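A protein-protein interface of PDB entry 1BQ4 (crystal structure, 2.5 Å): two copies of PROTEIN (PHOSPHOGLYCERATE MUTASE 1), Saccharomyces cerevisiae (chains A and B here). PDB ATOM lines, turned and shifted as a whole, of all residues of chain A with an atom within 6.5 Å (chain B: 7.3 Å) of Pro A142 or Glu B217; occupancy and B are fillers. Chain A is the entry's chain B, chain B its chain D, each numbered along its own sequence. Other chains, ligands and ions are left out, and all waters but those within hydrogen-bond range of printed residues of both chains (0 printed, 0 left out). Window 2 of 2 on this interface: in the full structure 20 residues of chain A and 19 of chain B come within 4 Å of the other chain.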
ATOM      1  N   LYS A 132       9.884 -26.793 -17.632  1.00  0.00           N
ATOM      2  CA  LYS A 132      11.244 -26.387 -17.945  1.00  0.00           C
ATOM      3  C   LYS A 132      11.117 -25.110 -18.778  1.00  0.00           C
ATOM      4  O   LYS A 132      10.606 -25.153 -19.906  1.00  0.00           O
ATOM      5  CB  LYS A 132      11.942 -27.494 -18.751  1.00  0.00           C
ATOM      6  CG  LYS A 132      13.406 -27.805 -18.359  1.00  0.00           C
ATOM      7  CD  LYS A 132      14.447 -26.870 -19.002  1.00  0.00           C
ATOM      8  CE  LYS A 132      15.914 -27.353 -18.785  1.00  0.00           C
ATOM      9  NZ  LYS A 132      16.517 -26.996 -17.458  1.00  0.00           N
ATOM     10  N   TYR A 137       9.043 -18.816 -13.453  1.00  0.00           N
ATOM     11  CA  TYR A 137      10.226 -19.379 -12.817  1.00  0.00           C
ATOM     12  C   TYR A 137      11.408 -18.879 -13.610  1.00  0.00           C
ATOM     13  O   TYR A 137      12.396 -19.557 -13.693  1.00  0.00           O
ATOM     14  CB  TYR A 137      10.177 -20.915 -12.871  1.00  0.00           C
ATOM     15  CG  TYR A 137       8.955 -21.548 -12.179  1.00  0.00           C
ATOM     16  CD1 TYR A 137       8.012 -22.288 -12.901  1.00  0.00           C
ATOM     17  CD2 TYR A 137       8.723 -21.355 -10.804  1.00  0.00           C
ATOM     18  CE1 TYR A 137       6.915 -22.797 -12.292  1.00  0.00           C
ATOM     19  CE2 TYR A 137       7.607 -21.861 -10.193  1.00  0.00           C
ATOM     20  CZ  TYR A 137       6.705 -22.587 -10.935  1.00  0.00           C
ATOM     21  OH  TYR A 137       5.606 -23.137 -10.300  1.00  0.00           O
ATOM     22  N   LYS A 138      11.341 -17.667 -14.157  1.00  0.00           N
ATOM     23  CA  LYS A 138      12.444 -17.197 -14.983  1.00  0.00           C
ATOM     24  C   LYS A 138      13.591 -16.491 -14.299  1.00  0.00           C
ATOM     25  O   LYS A 138      14.680 -16.393 -14.873  1.00  0.00           O
ATOM     26  CB  LYS A 138      11.940 -16.442 -16.244  1.00  0.00           C
ATOM     27  CG  LYS A 138      11.434 -15.009 -16.102  1.00  0.00           C
ATOM     28  CD  LYS A 138      11.311 -14.374 -17.496  1.00  0.00           C
ATOM     29  CE  LYS A 138      10.881 -12.894 -17.428  1.00  0.00           C
ATOM     30  NZ  LYS A 138      10.634 -12.213 -18.761  1.00  0.00           N
ATOM     31  N   VAL A 140      14.901 -17.535 -11.305  1.00  0.00           N
ATOM     32  CA  VAL A 140      15.401 -18.506 -10.330  1.00  0.00           C
ATOM     33  C   VAL A 140      16.501 -19.278 -11.041  1.00  0.00           C
ATOM     34  O   VAL A 140      16.432 -19.436 -12.263  1.00  0.00           O
ATOM     35  CB  VAL A 140      14.304 -19.523  -9.899  1.00  0.00           C
ATOM     36  CG1 VAL A 140      14.847 -20.470  -8.860  1.00  0.00           C
ATOM     37  CG2 VAL A 140      13.106 -18.804  -9.317  1.00  0.00           C
ATOM     38  N   ASP A 141      17.533 -19.692 -10.295  1.00  0.00           N
ATOM     39  CA  ASP A 141      18.661 -20.476 -10.823  1.00  0.00           C
ATOM     40  C   ASP A 141      18.091 -21.671 -11.601  1.00  0.00           C
ATOM     41  O   ASP A 141      17.548 -22.603 -11.007  1.00  0.00           O
ATOM     42  CB  ASP A 141      19.560 -20.958  -9.639  1.00  0.00           C
ATOM     43  CG  ASP A 141      20.761 -21.882 -10.060  1.00  0.00           C
ATOM     44  OD1 ASP A 141      21.081 -22.123 -11.263  1.00  0.00           O
ATOM     45  OD2 ASP A 141      21.428 -22.385  -9.124  1.00  0.00           O
ATOM     46  N   PRO A 142      18.201 -21.651 -12.943  1.00  0.00           N
ATOM     47  CA  PRO A 142      17.694 -22.760 -13.761  1.00  0.00           C
ATOM     48  C   PRO A 142      18.103 -24.135 -13.189  1.00  0.00           C
ATOM     49  O   PRO A 142      17.310 -25.076 -13.258  1.00  0.00           O
ATOM     50  CB  PRO A 142      18.369 -22.525 -15.129  1.00  0.00           C
ATOM     51  CG  PRO A 142      18.591 -21.108 -15.188  1.00  0.00           C
ATOM     52  CD  PRO A 142      18.951 -20.689 -13.777  1.00  0.00           C
ATOM     53  N   ASN A 143      19.308 -24.240 -12.614  1.00  0.00           N
ATOM     54  CA  ASN A 143      19.815 -25.502 -12.056  1.00  0.00           C
ATOM     55  C   ASN A 143      19.012 -26.110 -10.908  1.00  0.00           C
ATOM     56  O   ASN A 143      18.962 -27.338 -10.778  1.00  0.00           O
ATOM     57  CB  ASN A 143      21.264 -25.344 -11.585  1.00  0.00           C
ATOM     58  CG  ASN A 143      22.193 -24.967 -12.713  1.00  0.00           C
ATOM     59  OD1 ASN A 143      22.726 -25.846 -13.397  1.00  0.00           O
ATOM     60  ND2 ASN A 143      22.379 -23.643 -12.934  1.00  0.00           N
ATOM     61  N   VAL A 144      18.349 -25.275 -10.103  1.00  0.00           N
ATOM     62  CA  VAL A 144      17.603 -25.802  -8.962  1.00  0.00           C
ATOM     63  C   VAL A 144      16.142 -26.317  -9.180  1.00  0.00           C
ATOM     64  O   VAL A 144      15.585 -27.070  -8.333  1.00  0.00           O
ATOM     65  CB  VAL A 144      17.680 -24.826  -7.772  1.00  0.00           C
ATOM     66  CG1 VAL A 144      16.706 -23.578  -7.932  1.00  0.00           C
ATOM     67  CG2 VAL A 144      17.395 -25.592  -6.486  1.00  0.00           C
ATOM     68  N   LEU A 145      15.544 -25.887 -10.298  1.00  0.00           N
ATOM     69  CA  LEU A 145      14.195 -26.276 -10.686  1.00  0.00           C
ATOM     70  C   LEU A 145      14.157 -27.809 -10.832  1.00  0.00           C
ATOM     71  O   LEU A 145      15.008 -28.424 -11.503  1.00  0.00           O
ATOM     72  CB  LEU A 145      13.795 -25.541 -11.982  1.00  0.00           C
ATOM     73  CG  LEU A 145      13.050 -24.187 -11.833  1.00  0.00           C
ATOM     74  CD1 LEU A 145      13.281 -23.577 -10.499  1.00  0.00           C
ATOM     75  CD2 LEU A 145      13.389 -23.212 -12.954  1.00  0.00           C
ATOM     76  N   PRO A 146      13.213 -28.456 -10.135  1.00  0.00           N
ATOM     77  CA  PRO A 146      13.166 -29.909 -10.247  1.00  0.00           C
ATOM     78  C   PRO A 146      12.406 -30.344 -11.472  1.00  0.00           C
ATOM     79  O   PRO A 146      11.615 -29.582 -12.046  1.00  0.00           O
ATOM     80  CB  PRO A 146      12.403 -30.305  -9.002  1.00  0.00           C
ATOM     81  CG  PRO A 146      11.306 -29.270  -9.037  1.00  0.00           C
ATOM     82  CD  PRO A 146      12.064 -27.959  -9.345  1.00  0.00           C
ATOM     83  N   PRO B   1      25.188 -12.400 -17.761  1.00  0.00           N
ATOM     84  CA  PRO B   1      25.382 -12.263 -16.298  1.00  0.00           C
ATOM     85  C   PRO B   1      26.865 -12.169 -15.892  1.00  0.00           C
ATOM     86  O   PRO B   1      27.619 -13.141 -16.067  1.00  0.00           O
ATOM     87  CB  PRO B   1      24.750 -13.494 -15.643  1.00  0.00           C
ATOM     88  CG  PRO B   1      23.778 -13.996 -16.729  1.00  0.00           C
ATOM     89  CD  PRO B   1      24.394 -13.606 -18.080  1.00  0.00           C
ATOM     90  N   GLN B 163      20.449 -19.146  -5.557  1.00  0.00           N
ATOM     91  CA  GLN B 163      19.353 -19.677  -6.351  1.00  0.00           C
ATOM     92  C   GLN B 163      18.233 -18.686  -6.548  1.00  0.00           C
ATOM     93  O   GLN B 163      17.879 -18.389  -7.695  1.00  0.00           O
ATOM     94  CB  GLN B 163      18.840 -20.948  -5.681  1.00  0.00           C
ATOM     95  CG  GLN B 163      19.658 -22.159  -6.103  1.00  0.00           C
ATOM     96  CD  GLN B 163      19.680 -23.330  -5.123  1.00  0.00           C
ATOM     97  OE1 GLN B 163      18.958 -23.352  -4.123  1.00  0.00           O
ATOM     98  NE2 GLN B 163      20.521 -24.335  -5.432  1.00  0.00           N
ATOM     99  N   ALA B 167      20.806 -14.794  -8.109  1.00  0.00           N
ATOM    100  CA  ALA B 167      20.399 -15.117  -9.479  1.00  0.00           C
ATOM    101  C   ALA B 167      19.290 -14.240 -10.123  1.00  0.00           C
ATOM    102  O   ALA B 167      19.295 -14.047 -11.353  1.00  0.00           O
ATOM    103  CB  ALA B 167      20.013 -16.537  -9.531  1.00  0.00           C
ATOM    104  N   LEU B 171      20.089 -12.931 -13.571  1.00  0.00           N
ATOM    105  CA  LEU B 171      19.175 -13.201 -14.661  1.00  0.00           C
ATOM    106  C   LEU B 171      18.455 -11.913 -15.141  1.00  0.00           C
ATOM    107  O   LEU B 171      18.185 -11.762 -16.341  1.00  0.00           O
ATOM    108  CB  LEU B 171      18.212 -14.282 -14.258  1.00  0.00           C
ATOM    109  CG  LEU B 171      18.867 -15.654 -14.106  1.00  0.00           C
ATOM    110  CD1 LEU B 171      17.936 -16.585 -13.415  1.00  0.00           C
ATOM    111  CD2 LEU B 171      19.291 -16.219 -15.469  1.00  0.00           C
ATOM    112  N   LEU B 215      28.939 -15.682 -16.866  1.00  0.00           N
ATOM    113  CA  LEU B 215      27.939 -16.718 -16.840  1.00  0.00           C
ATOM    114  C   LEU B 215      27.024 -16.666 -18.032  1.00  0.00           C
ATOM    115  O   LEU B 215      26.824 -15.607 -18.599  1.00  0.00           O
ATOM    116  CB  LEU B 215      27.165 -16.557 -15.528  1.00  0.00           C
ATOM    117  CG  LEU B 215      28.052 -16.431 -14.274  1.00  0.00           C
ATOM    118  CD1 LEU B 215      27.300 -16.102 -12.993  1.00  0.00           C
ATOM    119  CD2 LEU B 215      28.779 -17.768 -14.099  1.00  0.00           C
ATOM    120  N   ASP B 216      26.519 -17.829 -18.437  1.00  0.00           N
ATOM    121  CA  ASP B 216      25.577 -17.924 -19.553  1.00  0.00           C
ATOM    122  C   ASP B 216      24.144 -17.889 -19.012  1.00  0.00           C
ATOM    123  O   ASP B 216      23.934 -17.664 -17.815  1.00  0.00           O
ATOM    124  CB  ASP B 216      25.813 -19.213 -20.366  1.00  0.00           C
ATOM    125  CG  ASP B 216      25.606 -20.487 -19.563  1.00  0.00           C
ATOM    126  OD1 ASP B 216      25.806 -21.581 -20.135  1.00  0.00           O
ATOM    127  OD2 ASP B 216      25.274 -20.404 -18.369  1.00  0.00           O
ATOM    128  N   GLU B 217      23.176 -18.156 -19.887  1.00  0.00           N
ATOM    129  CA  GLU B 217      21.762 -18.169 -19.498  1.00  0.00           C
ATOM    130  C   GLU B 217      21.476 -19.152 -18.336  1.00  0.00           C
ATOM    131  O   GLU B 217      20.531 -18.935 -17.577  1.00  0.00           O
ATOM    132  CB  GLU B 217      20.858 -18.366 -20.741  1.00  0.00           C
ATOM    133  CG  GLU B 217      20.182 -19.743 -20.966  1.00  0.00           C
ATOM    134  CD  GLU B 217      21.048 -20.823 -21.654  1.00  0.00           C
ATOM    135  OE1 GLU B 217      20.891 -22.011 -21.296  1.00  0.00           O
ATOM    136  OE2 GLU B 217      21.846 -20.515 -22.569  1.00  0.00           O
ATOM    137  N   ASN B 218      22.355 -20.156 -18.147  1.00  0.00           N
ATOM    138  CA  ASN B 218      22.262 -21.181 -17.067  1.00  0.00           C
ATOM    139  C   ASN B 218      23.123 -20.843 -15.811  1.00  0.00           C
ATOM    140  O   ASN B 218      23.301 -21.720 -14.947  1.00  0.00           O
ATOM    141  CB  ASN B 218      22.792 -22.566 -17.517  1.00  0.00           C
ATOM    142  CG  ASN B 218      21.916 -23.292 -18.540  1.00  0.00           C
ATOM    143  OD1 ASN B 218      20.872 -23.846 -18.203  1.00  0.00           O
ATOM    144  ND2 ASN B 218      22.435 -23.434 -19.755  1.00  0.00           N
ATOM    145  N   LEU B 219      23.696 -19.636 -15.732  1.00  0.00           N
ATOM    146  CA  LEU B 219      24.558 -19.255 -14.612  1.00  0.00           C
ATOM    147  C   LEU B 219      25.725 -20.266 -14.400  1.00  0.00           C
ATOM    148  O   LEU B 219      26.126 -20.626 -13.268  1.00  0.00           O
ATOM    149  CB  LEU B 219      23.752 -19.034 -13.340  1.00  0.00           C
ATOM    150  CG  LEU B 219      22.654 -17.950 -13.464  1.00  0.00           C
ATOM    151  CD1 LEU B 219      21.801 -17.928 -12.237  1.00  0.00           C
ATOM    152  CD2 LEU B 219      23.264 -16.595 -13.708  1.00  0.00           C
ATOM    153  N   LYS B 220      26.212 -20.745 -15.542  1.00  0.00           N
ATOM    154  CA  LYS B 220      27.324 -21.654 -15.639  1.00  0.00           C
ATOM    155  C   LYS B 220      28.293 -20.783 -16.442  1.00  0.00           C
ATOM    156  O   LYS B 220      27.855 -19.907 -17.202  1.00  0.00           O
ATOM    157  CB  LYS B 220      26.948 -22.901 -16.463  1.00  0.00           C
ATOM    158  CG  LYS B 220      26.346 -24.057 -15.651  1.00  0.00           C
ATOM    159  CD  LYS B 220      27.421 -24.961 -15.019  1.00  0.00           C
ATOM    160  CE  LYS B 220      26.830 -25.840 -13.907  1.00  0.00           C
ATOM    161  NZ  LYS B 220      26.480 -25.028 -12.694  1.00  0.00           N
ATOM    162  N   SER B 222      30.846 -19.137 -19.037  1.00  0.00           N
ATOM    163  CA  SER B 222      30.837 -19.016 -20.492  1.00  0.00           C
ATOM    164  C   SER B 222      32.279 -19.110 -21.003  1.00  0.00           C
ATOM    165  O   SER B 222      32.539 -19.567 -22.125  1.00  0.00           O
ATOM    166  CB  SER B 222      30.211 -17.665 -20.894  1.00  0.00           C
ATOM    167  OG  SER B 222      30.895 -16.561 -20.314  1.00  0.00           O
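The backbone carbonyl oxygen of Gln B163 lies within hydrogen-bond range of the backbone NH of Asp A141 (2.9 Å).
The backbone carbonyl oxygen of Asn B218 sits at hydrogen-bond distance from the side-chain amide nitrogen of Asn A143, 2.9 Å away.
OD2 of Asp B216 sits at hydrogen-bond distance from N of Asn B218 (2.9 Å).
The side-chain carboxylate (OD2) of Asp B216 is in hydrogen-bond range of the backbone NH (N) of Lys B220, at 3.0 Å.
The side-chain carboxylate (OE1) of Glu B217 is in hydrogen-bond range of the side-chain amide nitrogen (ND2) of Asn B218 (2.6 Å).
OD1 of Asp A141 sits at hydrogen-bond distance from ND2 of Asn A143, at 2.6 Å.
Lys A138 touches Leu B171.
Gln B163 touches Val A140 (O to CA, 3.6 Å).
Val A140 touches Leu B171 (O to CD1, 3.4 Å).
CG of Pro A142 touches O of Glu B217, at 3.8 Å.
Asn A143 touches Lys B220.
Val A144 touches Gln B163.
Pro A142 touches one residue of chain B.
Of the printed residues of chain B, Val A140 touches Gln B163 (3.6 Å) and Leu B171 (3.4 Å).
Of the printed residues of chain B, Asn A143 touches Asn B218 (2.9 Å) and Lys B220 (3.9 Å).
Of the printed residues of chain A, Leu B171 touches Lys A138 (3.6 Å) and Val A140 (3.4 Å).
Printed residues of chain B within 4 Å of Val A144: Gln B163.
Pro B1 touches none of the printed residues of chain A.
The nearest residue of chain B that does not touch Pro A142 is Asn B218 (4.1 Å).
The nearest printed residue of chain A that does not touch Glu B217 is Val A140 (6.7 Å).
The nearest printed residue of chain A that does not touch Leu B171 is Pro A142 (4.2 Å).
Of the 10 printed residues of chain A, 6 touch a printed residue of chain B.
Printed residues of chain A that touch a printed residue of chain B: Lys A138, Val A140, Asp A141, Pro A142, Asn A143 and Val A144.
Hydrophobic or aromatic side chains of chain A that line the printed part of chain B: Val A140, Pro A142 and Val A144.
Printed residues of chain B that touch a printed residue of chain A: Gln B163, Leu B171, Glu B217, Asn B218 and Lys B220.
Hydrophobic or aromatic side chains of chain B that line the printed part of chain A: Leu B171.
No position is printed for both chains.
Of the 8 pairs that touch across the chains among the printed residues, none has its exchanged pair printed and touching as well.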
